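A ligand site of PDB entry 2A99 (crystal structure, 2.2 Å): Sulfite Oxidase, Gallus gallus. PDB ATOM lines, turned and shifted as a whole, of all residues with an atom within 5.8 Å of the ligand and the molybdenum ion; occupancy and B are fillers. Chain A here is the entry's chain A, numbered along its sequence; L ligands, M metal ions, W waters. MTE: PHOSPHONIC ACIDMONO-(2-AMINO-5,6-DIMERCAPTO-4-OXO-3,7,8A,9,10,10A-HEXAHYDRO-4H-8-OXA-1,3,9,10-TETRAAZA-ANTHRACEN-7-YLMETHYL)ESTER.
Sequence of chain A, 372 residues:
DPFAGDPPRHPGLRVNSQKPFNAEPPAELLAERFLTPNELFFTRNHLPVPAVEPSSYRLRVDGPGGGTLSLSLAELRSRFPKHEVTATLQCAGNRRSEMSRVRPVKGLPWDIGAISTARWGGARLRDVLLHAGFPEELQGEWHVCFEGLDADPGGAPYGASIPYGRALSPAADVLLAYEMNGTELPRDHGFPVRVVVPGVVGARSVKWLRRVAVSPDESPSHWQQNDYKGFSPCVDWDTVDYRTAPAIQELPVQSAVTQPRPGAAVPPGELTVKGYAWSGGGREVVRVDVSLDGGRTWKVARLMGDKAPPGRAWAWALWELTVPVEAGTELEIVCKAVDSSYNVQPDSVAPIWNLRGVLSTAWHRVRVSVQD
A ring nitrogen (ND1) of His 189 sits at hydrogen-bond distance from an oxygen (O3P) of the ligand, at 2.7 Å.
An oxygen (O2P) of the ligand lies close to the backbone carbonyl oxygen of Phe 42, at 2.6 Å.
The backbone carbonyl oxygen (O) of Ser 205 lies within hydrogen-bond range of a nitrogen (N8) of the ligand (3.0 Å).
An oxygen (O1P) of the ligand is in hydrogen-bond range of the backbone NH of Arg 44, 3.0 Å away.
N2 of the ligand lies within hydrogen-bond range of OD1 of Asp 150 (2.8 Å).
The backbone NH (N) of His 46 is in hydrogen-bond range of an oxygen (O4) of the ligand, at 2.9 Å.
The side-chain amino group of Lys 207 lies within salt-bridge range of an oxygen (O1P) of the ligand (2.8 Å).
ND1 of His 46 is in hydrogen-bond range of O4 of the ligand (2.6 Å).
The guanidinium group (NE) of Arg 44 lies close to a sulfur (S1') of the ligand (3.6 Å).
The backbone carbonyl oxygen of Lys 207 lies within hydrogen-bond range of a nitrogen (N2) of the ligand.
N1 of the ligand is in hydrogen-bond range of N of Lys 207 (2.9 Å).
The guanidinium group (NH1) of Arg 194 is in salt-bridge range of an oxygen (O3P) of the ligand (2.8 Å).
OH of Tyr 228 sits close to S1' of the ligand.
The backbone carbonyl oxygen (O) of Arg 44 is in hydrogen-bond range of a nitrogen (N5) of the ligand, at 3.3 Å.
N of Leu 149 sits at hydrogen-bond distance from O of Trp 208 (2.8 Å).
The side-chain hydroxyl of Tyr 228 lies within hydrogen-bond range of a ring nitrogen (NE2) of His 46, at 2.9 Å.
O of Asp 150 is in hydrogen-bond range of N of Tyr 158, 2.9 Å away.
The side-chain carboxylate (OD1) of Asp 188 sits at hydrogen-bond distance from the side-chain amide nitrogen (ND2) of Asn 45 (3.2 Å).
The side-chain amino group (NZ) of Lys 207 lies within hydrogen-bond range of the backbone carbonyl oxygen (O) of Asp 188, 3.0 Å away.
SG of Cys 91 sits close to N of Gly 93 (3.5 Å).
NE2 of His 46 lies within hydrogen-bond range of NH2 of Arg 44, 3.5 Å away.
O of Ala 203 lies within hydrogen-bond range of OH of Tyr 158, at 2.6 Å.
Phe 41 touches the ligand (CE1 to O2P, 3.5 Å).
CA of Thr 43 touches O1P of the ligand (3.5 Å).
Asn 45 touches the ligand.
Tyr 158 touches the ligand (CD2 to N1, 3.3 Å).
O of Gly 202 touches C7 of the ligand, at 3.4 Å.
Ala 203 touches the ligand (CA to C1', 3.5 Å).
Val 206 touches the ligand.
Trp 208 touches the ligand (CE3 to N2, 3.4 Å).
Hydrophobic or aromatic side chains that line the ligand: Phe 41, Phe 42, His 46, Tyr 158, His 189, Ala 203, Val 206, Trp 208 and Tyr 228.
N of Ala 92 touches the molybdenum ion (3.9 Å).
The molybdenum ion is bound by water W3 (1.7 Å), a sulfur (S1') of the ligand (2.3 Å), water W1 (2.4 Å), a sulfur (S2') of the ligand (2.4 Å) and the side-chain sulfur of Cys 91 (2.5 Å).
The molybdenum ion has five donor atoms within binding distance.
Water W3 lies within hydrogen-bond range of N of Ala 92 and N of Ala 203.
Water W2 lies within hydrogen-bond range of OD2 of Asp 150, N of Leu 47, N of His 46 and O4 of the ligand.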
ATOM      1  N   PHE A  41       0.560   3.693   5.295  1.00  0.00           N
ATOM      2  CA  PHE A  41       0.915   2.904   6.467  1.00  0.00           C
ATOM      3  C   PHE A  41      -0.190   3.109   7.516  1.00  0.00           C
ATOM      4  O   PHE A  41      -0.593   4.237   7.775  1.00  0.00           O
ATOM      5  CB  PHE A  41       2.272   3.389   7.000  1.00  0.00           C
ATOM      6  CG  PHE A  41       2.947   2.423   7.896  1.00  0.00           C
ATOM      7  CD1 PHE A  41       2.526   2.243   9.220  1.00  0.00           C
ATOM      8  CD2 PHE A  41       4.046   1.732   7.457  1.00  0.00           C
ATOM      9  CE1 PHE A  41       3.169   1.387  10.046  1.00  0.00           C
ATOM     10  CE2 PHE A  41       4.702   0.823   8.310  1.00  0.00           C
ATOM     11  CZ  PHE A  41       4.277   0.675   9.604  1.00  0.00           C
ATOM     12  N   PHE A  42      -0.702   2.024   8.087  1.00  0.00           N
ATOM     13  CA  PHE A  42      -1.822   2.146   9.029  1.00  0.00           C
ATOM     14  C   PHE A  42      -1.395   3.033  10.173  1.00  0.00           C
ATOM     15  O   PHE A  42      -0.228   3.077  10.552  1.00  0.00           O
ATOM     16  CB  PHE A  42      -2.358   0.792   9.532  1.00  0.00           C
ATOM     17  CG  PHE A  42      -1.676   0.273  10.753  1.00  0.00           C
ATOM     18  CD1 PHE A  42      -0.446  -0.370  10.679  1.00  0.00           C
ATOM     19  CD2 PHE A  42      -2.280   0.360  11.982  1.00  0.00           C
ATOM     20  CE1 PHE A  42       0.171  -0.873  11.840  1.00  0.00           C
ATOM     21  CE2 PHE A  42      -1.667  -0.134  13.106  1.00  0.00           C
ATOM     22  CZ  PHE A  42      -0.441  -0.735  13.032  1.00  0.00           C
ATOM     23  N   THR A  43      -2.380   3.732  10.707  1.00  0.00           N
ATOM     24  CA  THR A  43      -2.168   4.688  11.778  1.00  0.00           C
ATOM     25  C   THR A  43      -3.082   4.377  12.950  1.00  0.00           C
ATOM     26  O   THR A  43      -4.298   4.206  12.790  1.00  0.00           O
ATOM     27  CB  THR A  43      -2.436   6.094  11.282  1.00  0.00           C
ATOM     28  OG1 THR A  43      -1.560   6.358  10.194  1.00  0.00           O
ATOM     29  CG2 THR A  43      -2.146   7.106  12.358  1.00  0.00           C
ATOM     30  N   ARG A  44      -2.448   4.191  14.099  1.00  0.00           N
ATOM     31  CA  ARG A  44      -3.128   3.942  15.333  1.00  0.00           C
ATOM     32  C   ARG A  44      -2.666   4.944  16.398  1.00  0.00           C
ATOM     33  O   ARG A  44      -1.568   4.824  16.963  1.00  0.00           O
ATOM     34  CB  ARG A  44      -2.859   2.503  15.793  1.00  0.00           C
ATOM     35  CG  ARG A  44      -3.864   1.952  16.779  1.00  0.00           C
ATOM     36  CD  ARG A  44      -3.762   2.594  18.142  1.00  0.00           C
ATOM     37  NE  ARG A  44      -4.649   1.925  19.101  1.00  0.00           N
ATOM     38  CZ  ARG A  44      -5.745   2.466  19.608  1.00  0.00           C
ATOM     39  NH1 ARG A  44      -6.122   3.712  19.315  1.00  0.00           N
ATOM     40  NH2 ARG A  44      -6.450   1.770  20.465  1.00  0.00           N
ATOM     41  N   ASN A  45      -3.533   5.924  16.661  1.00  0.00           N
ATOM     42  CA  ASN A  45      -3.323   6.974  17.655  1.00  0.00           C
ATOM     43  C   ASN A  45      -4.300   6.838  18.818  1.00  0.00           C
ATOM     44  O   ASN A  45      -5.501   6.690  18.615  1.00  0.00           O
ATOM     45  CB  ASN A  45      -3.567   8.362  17.019  1.00  0.00           C
ATOM     46  CG  ASN A  45      -2.568   8.705  15.937  1.00  0.00           C
ATOM     47  OD1 ASN A  45      -1.579   8.009  15.774  1.00  0.00           O
ATOM     48  ND2 ASN A  45      -2.818   9.798  15.203  1.00  0.00           N
ATOM     49  N   HIS A  46      -3.812   6.874  20.037  1.00  0.00           N
ATOM     50  CA  HIS A  46      -4.718   6.869  21.208  1.00  0.00           C
ATOM     51  C   HIS A  46      -5.122   8.280  21.566  1.00  0.00           C
ATOM     52  O   HIS A  46      -6.144   8.500  22.195  1.00  0.00           O
ATOM     53  CB  HIS A  46      -4.057   6.281  22.437  1.00  0.00           C
ATOM     54  CG  HIS A  46      -3.877   4.790  22.386  1.00  0.00           C
ATOM     55  ND1 HIS A  46      -2.819   4.193  21.736  1.00  0.00           N
ATOM     56  CD2 HIS A  46      -4.554   3.792  22.995  1.00  0.00           C
ATOM     57  CE1 HIS A  46      -2.899   2.884  21.896  1.00  0.00           C
ATOM     58  NE2 HIS A  46      -3.925   2.616  22.667  1.00  0.00           N
ATOM     59  N   LEU A  47      -4.355   9.243  21.073  1.00  0.00           N
ATOM     60  CA  LEU A  47      -4.507  10.630  21.508  1.00  0.00           C
ATOM     61  C   LEU A  47      -4.234  11.621  20.391  1.00  0.00           C
ATOM     62  O   LEU A  47      -3.975  11.230  19.256  1.00  0.00           O
ATOM     63  CB  LEU A  47      -3.495  10.854  22.660  1.00  0.00           C
ATOM     64  CG  LEU A  47      -3.772  10.006  23.918  1.00  0.00           C
ATOM     65  CD1 LEU A  47      -2.576   9.958  24.818  1.00  0.00           C
ATOM     66  CD2 LEU A  47      -5.027  10.520  24.710  1.00  0.00           C
ATOM     67  N   LEU A  89       4.893  -3.691  11.558  1.00  0.00           N
ATOM     68  CA  LEU A  89       4.156  -3.384  12.774  1.00  0.00           C
ATOM     69  C   LEU A  89       2.729  -3.855  12.507  1.00  0.00           C
ATOM     70  O   LEU A  89       2.171  -3.540  11.422  1.00  0.00           O
ATOM     71  CB  LEU A  89       4.155  -1.874  13.062  1.00  0.00           C
ATOM     72  CG  LEU A  89       5.532  -1.196  13.275  1.00  0.00           C
ATOM     73  CD1 LEU A  89       5.369   0.257  13.625  1.00  0.00           C
ATOM     74  CD2 LEU A  89       6.209  -1.915  14.388  1.00  0.00           C
ATOM     75  N   GLN A  90       2.227  -4.661  13.453  1.00  0.00           N
ATOM     76  CA  GLN A  90       0.881  -5.180  13.466  1.00  0.00           C
ATOM     77  C   GLN A  90       0.270  -4.823  14.794  1.00  0.00           C
ATOM     78  O   GLN A  90       0.872  -5.028  15.849  1.00  0.00           O
ATOM     79  CB  GLN A  90       0.838  -6.717  13.365  1.00  0.00           C
ATOM     80  CG  GLN A  90      -0.584  -7.203  13.178  1.00  0.00           C
ATOM     81  CD  GLN A  90      -0.759  -8.685  13.157  1.00  0.00           C
ATOM     82  OE1 GLN A  90       0.194  -9.485  13.332  1.00  0.00           O
ATOM     83  NE2 GLN A  90      -1.971  -9.090  12.943  1.00  0.00           N
ATOM     84  N   CYS A  91      -0.918  -4.279  14.732  1.00  0.00           N
ATOM     85  CA  CYS A  91      -1.659  -3.963  15.913  1.00  0.00           C
ATOM     86  C   CYS A  91      -2.285  -5.219  16.523  1.00  0.00           C
ATOM     87  O   CYS A  91      -2.689  -6.142  15.810  1.00  0.00           O
ATOM     88  CB  CYS A  91      -2.723  -2.896  15.548  1.00  0.00           C
ATOM     89  SG  CYS A  91      -3.701  -2.291  16.913  1.00  0.00           S
ATOM     90  N   ALA A  92      -2.399  -5.224  17.856  1.00  0.00           N
ATOM     91  CA  ALA A  92      -3.018  -6.312  18.573  1.00  0.00           C
ATOM     92  C   ALA A  92      -4.445  -6.496  18.087  1.00  0.00           C
ATOM     93  O   ALA A  92      -4.970  -7.618  18.094  1.00  0.00           O
ATOM     94  CB  ALA A  92      -2.996  -6.031  20.066  1.00  0.00           C
ATOM     95  N   GLY A  93      -5.058  -5.393  17.685  1.00  0.00           N
ATOM     96  CA  GLY A  93      -6.460  -5.389  17.253  1.00  0.00           C
ATOM     97  C   GLY A  93      -6.723  -5.702  15.799  1.00  0.00           C
ATOM     98  O   GLY A  93      -7.853  -5.648  15.357  1.00  0.00           O
ATOM     99  N   TRP A 120      12.944   1.231   8.529  1.00  0.00           N
ATOM    100  CA  TRP A 120      13.151   2.236   9.554  1.00  0.00           C
ATOM    101  C   TRP A 120      14.632   2.555   9.713  1.00  0.00           C
ATOM    102  O   TRP A 120      15.465   1.647   9.596  1.00  0.00           O
ATOM    103  CB  TRP A 120      12.622   1.689  10.879  1.00  0.00           C
ATOM    104  CG  TRP A 120      11.209   1.185  10.798  1.00  0.00           C
ATOM    105  CD1 TRP A 120      10.805  -0.117  10.652  1.00  0.00           C
ATOM    106  CD2 TRP A 120      10.005   1.960  10.918  1.00  0.00           C
ATOM    107  NE1 TRP A 120       9.443  -0.198  10.656  1.00  0.00           N
ATOM    108  CE2 TRP A 120       8.920   1.069  10.807  1.00  0.00           C
ATOM    109  CE3 TRP A 120       9.742   3.322  11.077  1.00  0.00           C
ATOM    110  CZ2 TRP A 120       7.601   1.486  10.867  1.00  0.00           C
ATOM    111  CZ3 TRP A 120       8.432   3.743  11.139  1.00  0.00           C
ATOM    112  CH2 TRP A 120       7.369   2.834  11.052  1.00  0.00           C
ATOM    113  N   GLY A 148       5.580   8.545  25.726  1.00  0.00           N
ATOM    114  CA  GLY A 148       5.412   9.413  24.572  1.00  0.00           C
ATOM    115  C   GLY A 148       5.025  10.826  25.022  1.00  0.00           C
ATOM    116  O   GLY A 148       4.755  11.057  26.211  1.00  0.00           O
ATOM    117  N   LEU A 149       5.061  11.763  24.070  1.00  0.00           N
ATOM    118  CA  LEU A 149       4.728  13.149  24.328  1.00  0.00           C
ATOM    119  C   LEU A 149       3.228  13.372  24.344  1.00  0.00           C
ATOM    120  O   LEU A 149       2.770  14.416  24.787  1.00  0.00           O
ATOM    121  CB  LEU A 149       5.370  14.078  23.274  1.00  0.00           C
ATOM    122  CG  LEU A 149       6.865  14.319  23.446  1.00  0.00           C
ATOM    123  CD1 LEU A 149       7.475  14.784  22.137  1.00  0.00           C
ATOM    124  CD2 LEU A 149       7.094  15.331  24.542  1.00  0.00           C
ATOM    125  N   ASP A 150       2.468  12.380  23.885  1.00  0.00           N
ATOM    126  CA  ASP A 150       1.007  12.439  23.899  1.00  0.00           C
ATOM    127  C   ASP A 150       0.465  11.995  25.250  1.00  0.00           C
ATOM    128  O   ASP A 150       0.855  10.958  25.772  1.00  0.00           O
ATOM    129  CB  ASP A 150       0.406  11.642  22.746  1.00  0.00           C
ATOM    130  CG  ASP A 150       0.830  10.177  22.735  1.00  0.00           C
ATOM    131  OD1 ASP A 150       1.984   9.869  23.112  1.00  0.00           O
ATOM    132  OD2 ASP A 150       0.022   9.336  22.247  1.00  0.00           O
ATOM    133  N   TYR A 158       1.175   8.271  26.896  1.00  0.00           N
ATOM    134  CA  TYR A 158       1.123   6.924  26.388  1.00  0.00           C
ATOM    135  C   TYR A 158       2.463   6.327  26.758  1.00  0.00           C
ATOM    136  O   TYR A 158       3.477   7.003  26.739  1.00  0.00           O
ATOM    137  CB  TYR A 158       0.873   6.825  24.878  1.00  0.00           C
ATOM    138  CG  TYR A 158       0.808   5.375  24.433  1.00  0.00           C
ATOM    139  CD1 TYR A 158      -0.348   4.619  24.592  1.00  0.00           C
ATOM    140  CD2 TYR A 158       1.936   4.739  23.937  1.00  0.00           C
ATOM    141  CE1 TYR A 158      -0.378   3.267  24.246  1.00  0.00           C
ATOM    142  CE2 TYR A 158       1.911   3.399  23.558  1.00  0.00           C
ATOM    143  CZ  TYR A 158       0.748   2.677  23.695  1.00  0.00           C
ATOM    144  OH  TYR A 158       0.761   1.334  23.342  1.00  0.00           O
ATOM    145  N   ASP A 188       2.131  11.587  12.100  1.00  0.00           N
ATOM    146  CA  ASP A 188       1.257  10.486  12.530  1.00  0.00           C
ATOM    147  C   ASP A 188       2.054   9.249  12.965  1.00  0.00           C
ATOM    148  O   ASP A 188       1.540   8.443  13.722  1.00  0.00           O
ATOM    149  CB  ASP A 188       0.306  10.055  11.393  1.00  0.00           C
ATOM    150  CG  ASP A 188      -1.067  10.692  11.470  1.00  0.00           C
ATOM    151  OD1 ASP A 188      -1.527  11.082  12.574  1.00  0.00           O
ATOM    152  OD2 ASP A 188      -1.721  10.716  10.405  1.00  0.00           O
ATOM    153  N   HIS A 189       3.313   9.127  12.499  1.00  0.00           N
ATOM    154  CA  HIS A 189       4.126   7.957  12.794  1.00  0.00           C
ATOM    155  C   HIS A 189       5.229   8.232  13.794  1.00  0.00           C
ATOM    156  O   HIS A 189       6.111   7.412  13.969  1.00  0.00           O
ATOM    157  CB  HIS A 189       4.627   7.300  11.505  1.00  0.00           C
ATOM    158  CG  HIS A 189       3.496   6.852  10.632  1.00  0.00           C
ATOM    159  ND1 HIS A 189       2.671   5.810  10.968  1.00  0.00           N
ATOM    160  CD2 HIS A 189       2.958   7.404   9.522  1.00  0.00           C
ATOM    161  CE1 HIS A 189       1.711   5.696  10.072  1.00  0.00           C
ATOM    162  NE2 HIS A 189       1.848   6.670   9.181  1.00  0.00           N
ATOM    163  N   ARG A 194      10.497   7.711  17.279  1.00  0.00           N
ATOM    164  CA  ARG A 194       9.691   6.628  17.871  1.00  0.00           C
ATOM    165  C   ARG A 194      10.574   5.407  18.182  1.00  0.00           C
ATOM    166  O   ARG A 194      11.637   5.273  17.646  1.00  0.00           O
ATOM    167  CB  ARG A 194       8.592   6.169  16.904  1.00  0.00           C
ATOM    168  CG  ARG A 194       9.117   5.234  15.774  1.00  0.00           C
ATOM    169  CD  ARG A 194       8.011   4.647  14.921  1.00  0.00           C
ATOM    170  NE  ARG A 194       7.045   3.885  15.696  1.00  0.00           N
ATOM    171  CZ  ARG A 194       5.839   3.524  15.246  1.00  0.00           C
ATOM    172  NH1 ARG A 194       5.467   3.858  14.029  1.00  0.00           N
ATOM    173  NH2 ARG A 194       4.985   2.888  16.045  1.00  0.00           N
ATOM    174  N   VAL A 201       4.278  -6.697  19.191  1.00  0.00           N
ATOM    175  CA  VAL A 201       3.023  -5.989  18.957  1.00  0.00           C
ATOM    176  C   VAL A 201       3.269  -4.494  18.827  1.00  0.00           C
ATOM    177  O   VAL A 201       4.171  -3.928  19.457  1.00  0.00           O
ATOM    178  CB  VAL A 201       1.986  -6.312  20.032  1.00  0.00           C
ATOM    179  CG1 VAL A 201       2.373  -5.757  21.357  1.00  0.00           C
ATOM    180  CG2 VAL A 201       0.622  -5.767  19.654  1.00  0.00           C
ATOM    181  N   GLY A 202       2.482  -3.876  17.959  1.00  0.00           N
ATOM    182  CA  GLY A 202       2.605  -2.461  17.627  1.00  0.00           C
ATOM    183  C   GLY A 202       2.570  -1.563  18.827  1.00  0.00           C
ATOM    184  O   GLY A 202       3.289  -0.611  18.865  1.00  0.00           O
ATOM    185  N   ALA A 203       1.785  -1.924  19.840  1.00  0.00           N
ATOM    186  CA  ALA A 203       1.650  -1.100  21.063  1.00  0.00           C
ATOM    187  C   ALA A 203       2.955  -0.709  21.784  1.00  0.00           C
ATOM    188  O   ALA A 203       2.964   0.278  22.522  1.00  0.00           O
ATOM    189  CB  ALA A 203       0.711  -1.788  22.072  1.00  0.00           C
ATOM    190  N   ARG A 204       4.031  -1.490  21.619  1.00  0.00           N
ATOM    191  CA  ARG A 204       5.271  -1.224  22.344  1.00  0.00           C
ATOM    192  C   ARG A 204       6.187  -0.245  21.577  1.00  0.00           C
ATOM    193  O   ARG A 204       7.104   0.319  22.158  1.00  0.00           O
ATOM    194  CB  ARG A 204       6.056  -2.523  22.669  1.00  0.00           C
ATOM    195  CG  ARG A 204       5.283  -3.725  23.300  1.00  0.00           C
ATOM    196  CD  ARG A 204       4.400  -3.330  24.410  1.00  0.00           C
ATOM    197  NE  ARG A 204       3.514  -4.408  24.852  1.00  0.00           N
ATOM    198  CZ  ARG A 204       2.347  -4.249  25.485  1.00  0.00           C
ATOM    199  NH1 ARG A 204       1.868  -3.038  25.827  1.00  0.00           N
ATOM    200  NH2 ARG A 204       1.638  -5.312  25.792  1.00  0.00           N
ATOM    201  N   SER A 205       5.919  -0.048  20.288  1.00  0.00           N
ATOM    202  CA  SER A 205       6.716   0.840  19.442  1.00  0.00           C
ATOM    203  C   SER A 205       6.213   2.258  19.674  1.00  0.00           C
ATOM    204  O   SER A 205       5.516   2.831  18.860  1.00  0.00           O
ATOM    205  CB  SER A 205       6.647   0.440  17.959  1.00  0.00           C
ATOM    206  OG  SER A 205       7.387  -0.745  17.675  1.00  0.00           O
ATOM    207  N   VAL A 206       6.600   2.807  20.815  1.00  0.00           N
ATOM    208  CA  VAL A 206       6.135   4.094  21.277  1.00  0.00           C
ATOM    209  C   VAL A 206       6.581   5.250  20.382  1.00  0.00           C
ATOM    210  O   VAL A 206       7.781   5.463  20.156  1.00  0.00           O
ATOM    211  CB  VAL A 206       6.599   4.343  22.733  1.00  0.00           C
ATOM    212  CG1 VAL A 206       6.261   5.771  23.187  1.00  0.00           C
ATOM    213  CG2 VAL A 206       5.948   3.327  23.661  1.00  0.00           C
ATOM    214  N   LYS A 207       5.599   6.016  19.931  1.00  0.00           N
ATOM    215  CA  LYS A 207       5.809   7.176  19.046  1.00  0.00           C
ATOM    216  C   LYS A 207       5.993   8.480  19.842  1.00  0.00           C
ATOM    217  O   LYS A 207       5.627   8.544  21.001  1.00  0.00           O
ATOM    218  CB  LYS A 207       4.584   7.334  18.143  1.00  0.00           C
ATOM    219  CG  LYS A 207       4.342   6.228  17.139  1.00  0.00           C
ATOM    220  CD  LYS A 207       3.169   6.494  16.186  1.00  0.00           C
ATOM    221  CE  LYS A 207       1.797   6.217  16.789  1.00  0.00           C
ATOM    222  NZ  LYS A 207       0.666   6.410  15.781  1.00  0.00           N
ATOM    223  N   TRP A 208       6.560   9.518  19.216  1.00  0.00           N
ATOM    224  CA  TRP A 208       6.737  10.837  19.864  1.00  0.00           C
ATOM    225  C   TRP A 208       7.453  10.664  21.215  1.00  0.00           C
ATOM    226  O   TRP A 208       7.074  11.249  22.249  1.00  0.00           O
ATOM    227  CB  TRP A 208       5.372  11.537  20.027  1.00  0.00           C
ATOM    228  CG  TRP A 208       4.510  11.511  18.788  1.00  0.00           C
ATOM    229  CD1 TRP A 208       4.729  12.209  17.619  1.00  0.00           C
ATOM    230  CD2 TRP A 208       3.272  10.793  18.603  1.00  0.00           C
ATOM    231  NE1 TRP A 208       3.739  11.918  16.709  1.00  0.00           N
ATOM    232  CE2 TRP A 208       2.830  11.064  17.287  1.00  0.00           C
ATOM    233  CE3 TRP A 208       2.527   9.901  19.392  1.00  0.00           C
ATOM    234  CZ2 TRP A 208       1.660  10.513  16.762  1.00  0.00           C
ATOM    235  CZ3 TRP A 208       1.381   9.346  18.865  1.00  0.00           C
ATOM    236  CH2 TRP A 208       0.979   9.628  17.551  1.00  0.00           C
ATOM    237  N   TYR A 228      -3.858  -4.656  26.172  1.00  0.00           N
ATOM    238  CA  TYR A 228      -2.937  -5.476  25.325  1.00  0.00           C
ATOM    239  C   TYR A 228      -2.530  -6.804  26.008  1.00  0.00           C
ATOM    240  O   TYR A 228      -1.336  -7.117  26.172  1.00  0.00           O
ATOM    241  CB  TYR A 228      -1.724  -4.657  24.846  1.00  0.00           C
ATOM    242  CG  TYR A 228      -2.182  -3.449  24.074  1.00  0.00           C
ATOM    243  CD1 TYR A 228      -2.887  -3.603  22.878  1.00  0.00           C
ATOM    244  CD2 TYR A 228      -2.039  -2.149  24.594  1.00  0.00           C
ATOM    245  CE1 TYR A 228      -3.456  -2.517  22.224  1.00  0.00           C
ATOM    246  CE2 TYR A 228      -2.565  -1.031  23.904  1.00  0.00           C
ATOM    247  CZ  TYR A 228      -3.295  -1.234  22.743  1.00  0.00           C
ATOM    248  OH  TYR A 228      -3.822  -0.163  22.042  1.00  0.00           O
HETATM  249  N1  MTE L   1       2.831   5.551  20.834  1.00  0.00           N
HETATM  250  C2  MTE L   1       2.266   6.673  21.242  1.00  0.00           C
HETATM  251  N2  MTE L   1       2.971   7.573  21.897  1.00  0.00           N
HETATM  252  N3  MTE L   1       0.901   6.757  21.350  1.00  0.00           N
HETATM  253  C4  MTE L   1       0.045   5.881  20.731  1.00  0.00           C
HETATM  254  O4  MTE L   1      -1.196   6.054  20.909  1.00  0.00           O
HETATM  255  N5  MTE L   1      -0.088   3.662  19.662  1.00  0.00           N
HETATM  256  C6  MTE L   1       0.497   2.426  19.680  1.00  0.00           C
HETATM  257  C7  MTE L   1       1.982   2.512  19.163  1.00  0.00           C
HETATM  258  N8  MTE L   1       2.685   3.608  19.686  1.00  0.00           N
HETATM  259  C9  MTE L   1       0.641   4.744  20.153  1.00  0.00           C
HETATM  260  C10 MTE L   1       2.055   4.678  20.157  1.00  0.00           C
HETATM  261  C1' MTE L   1      -0.044   1.258  19.070  1.00  0.00           C
HETATM  262  S1' MTE L   1      -1.419   0.447  19.870  1.00  0.00           S
HETATM  263  C2' MTE L   1       0.163   0.984  17.770  1.00  0.00           C
HETATM  264  S2' MTE L   1      -0.596  -0.442  17.019  1.00  0.00           S
HETATM  265  C3' MTE L   1       1.319   1.577  17.016  1.00  0.00           C
HETATM  266  O3' MTE L   1       1.926   2.657  17.703  1.00  0.00           O
HETATM  267  C4' MTE L   1       0.889   2.001  15.691  1.00  0.00           C
HETATM  268  O4' MTE L   1       1.917   2.674  14.926  1.00  0.00           O
HETATM  269  P   MTE L   1       1.569   3.398  13.585  1.00  0.00           P
HETATM  270  O1P MTE L   1       0.559   4.413  13.875  1.00  0.00           O
HETATM  271  O2P MTE L   1       1.113   2.382  12.634  1.00  0.00           O
HETATM  272  O3P MTE L   1       2.855   4.139  13.107  1.00  0.00           O
HETATM  273 MO    MO M   1      -2.099  -1.405  18.623  1.00  0.00          MO
HETATM  274  O   HOH W   1      -4.081  -0.793  19.822  1.00  0.00           O
HETATM  275  O   HOH W   2      -1.680   9.375  19.961  1.00  0.00           O
HETATM  276  O   HOH W   3      -1.315  -2.812  19.245  1.00  0.00           O
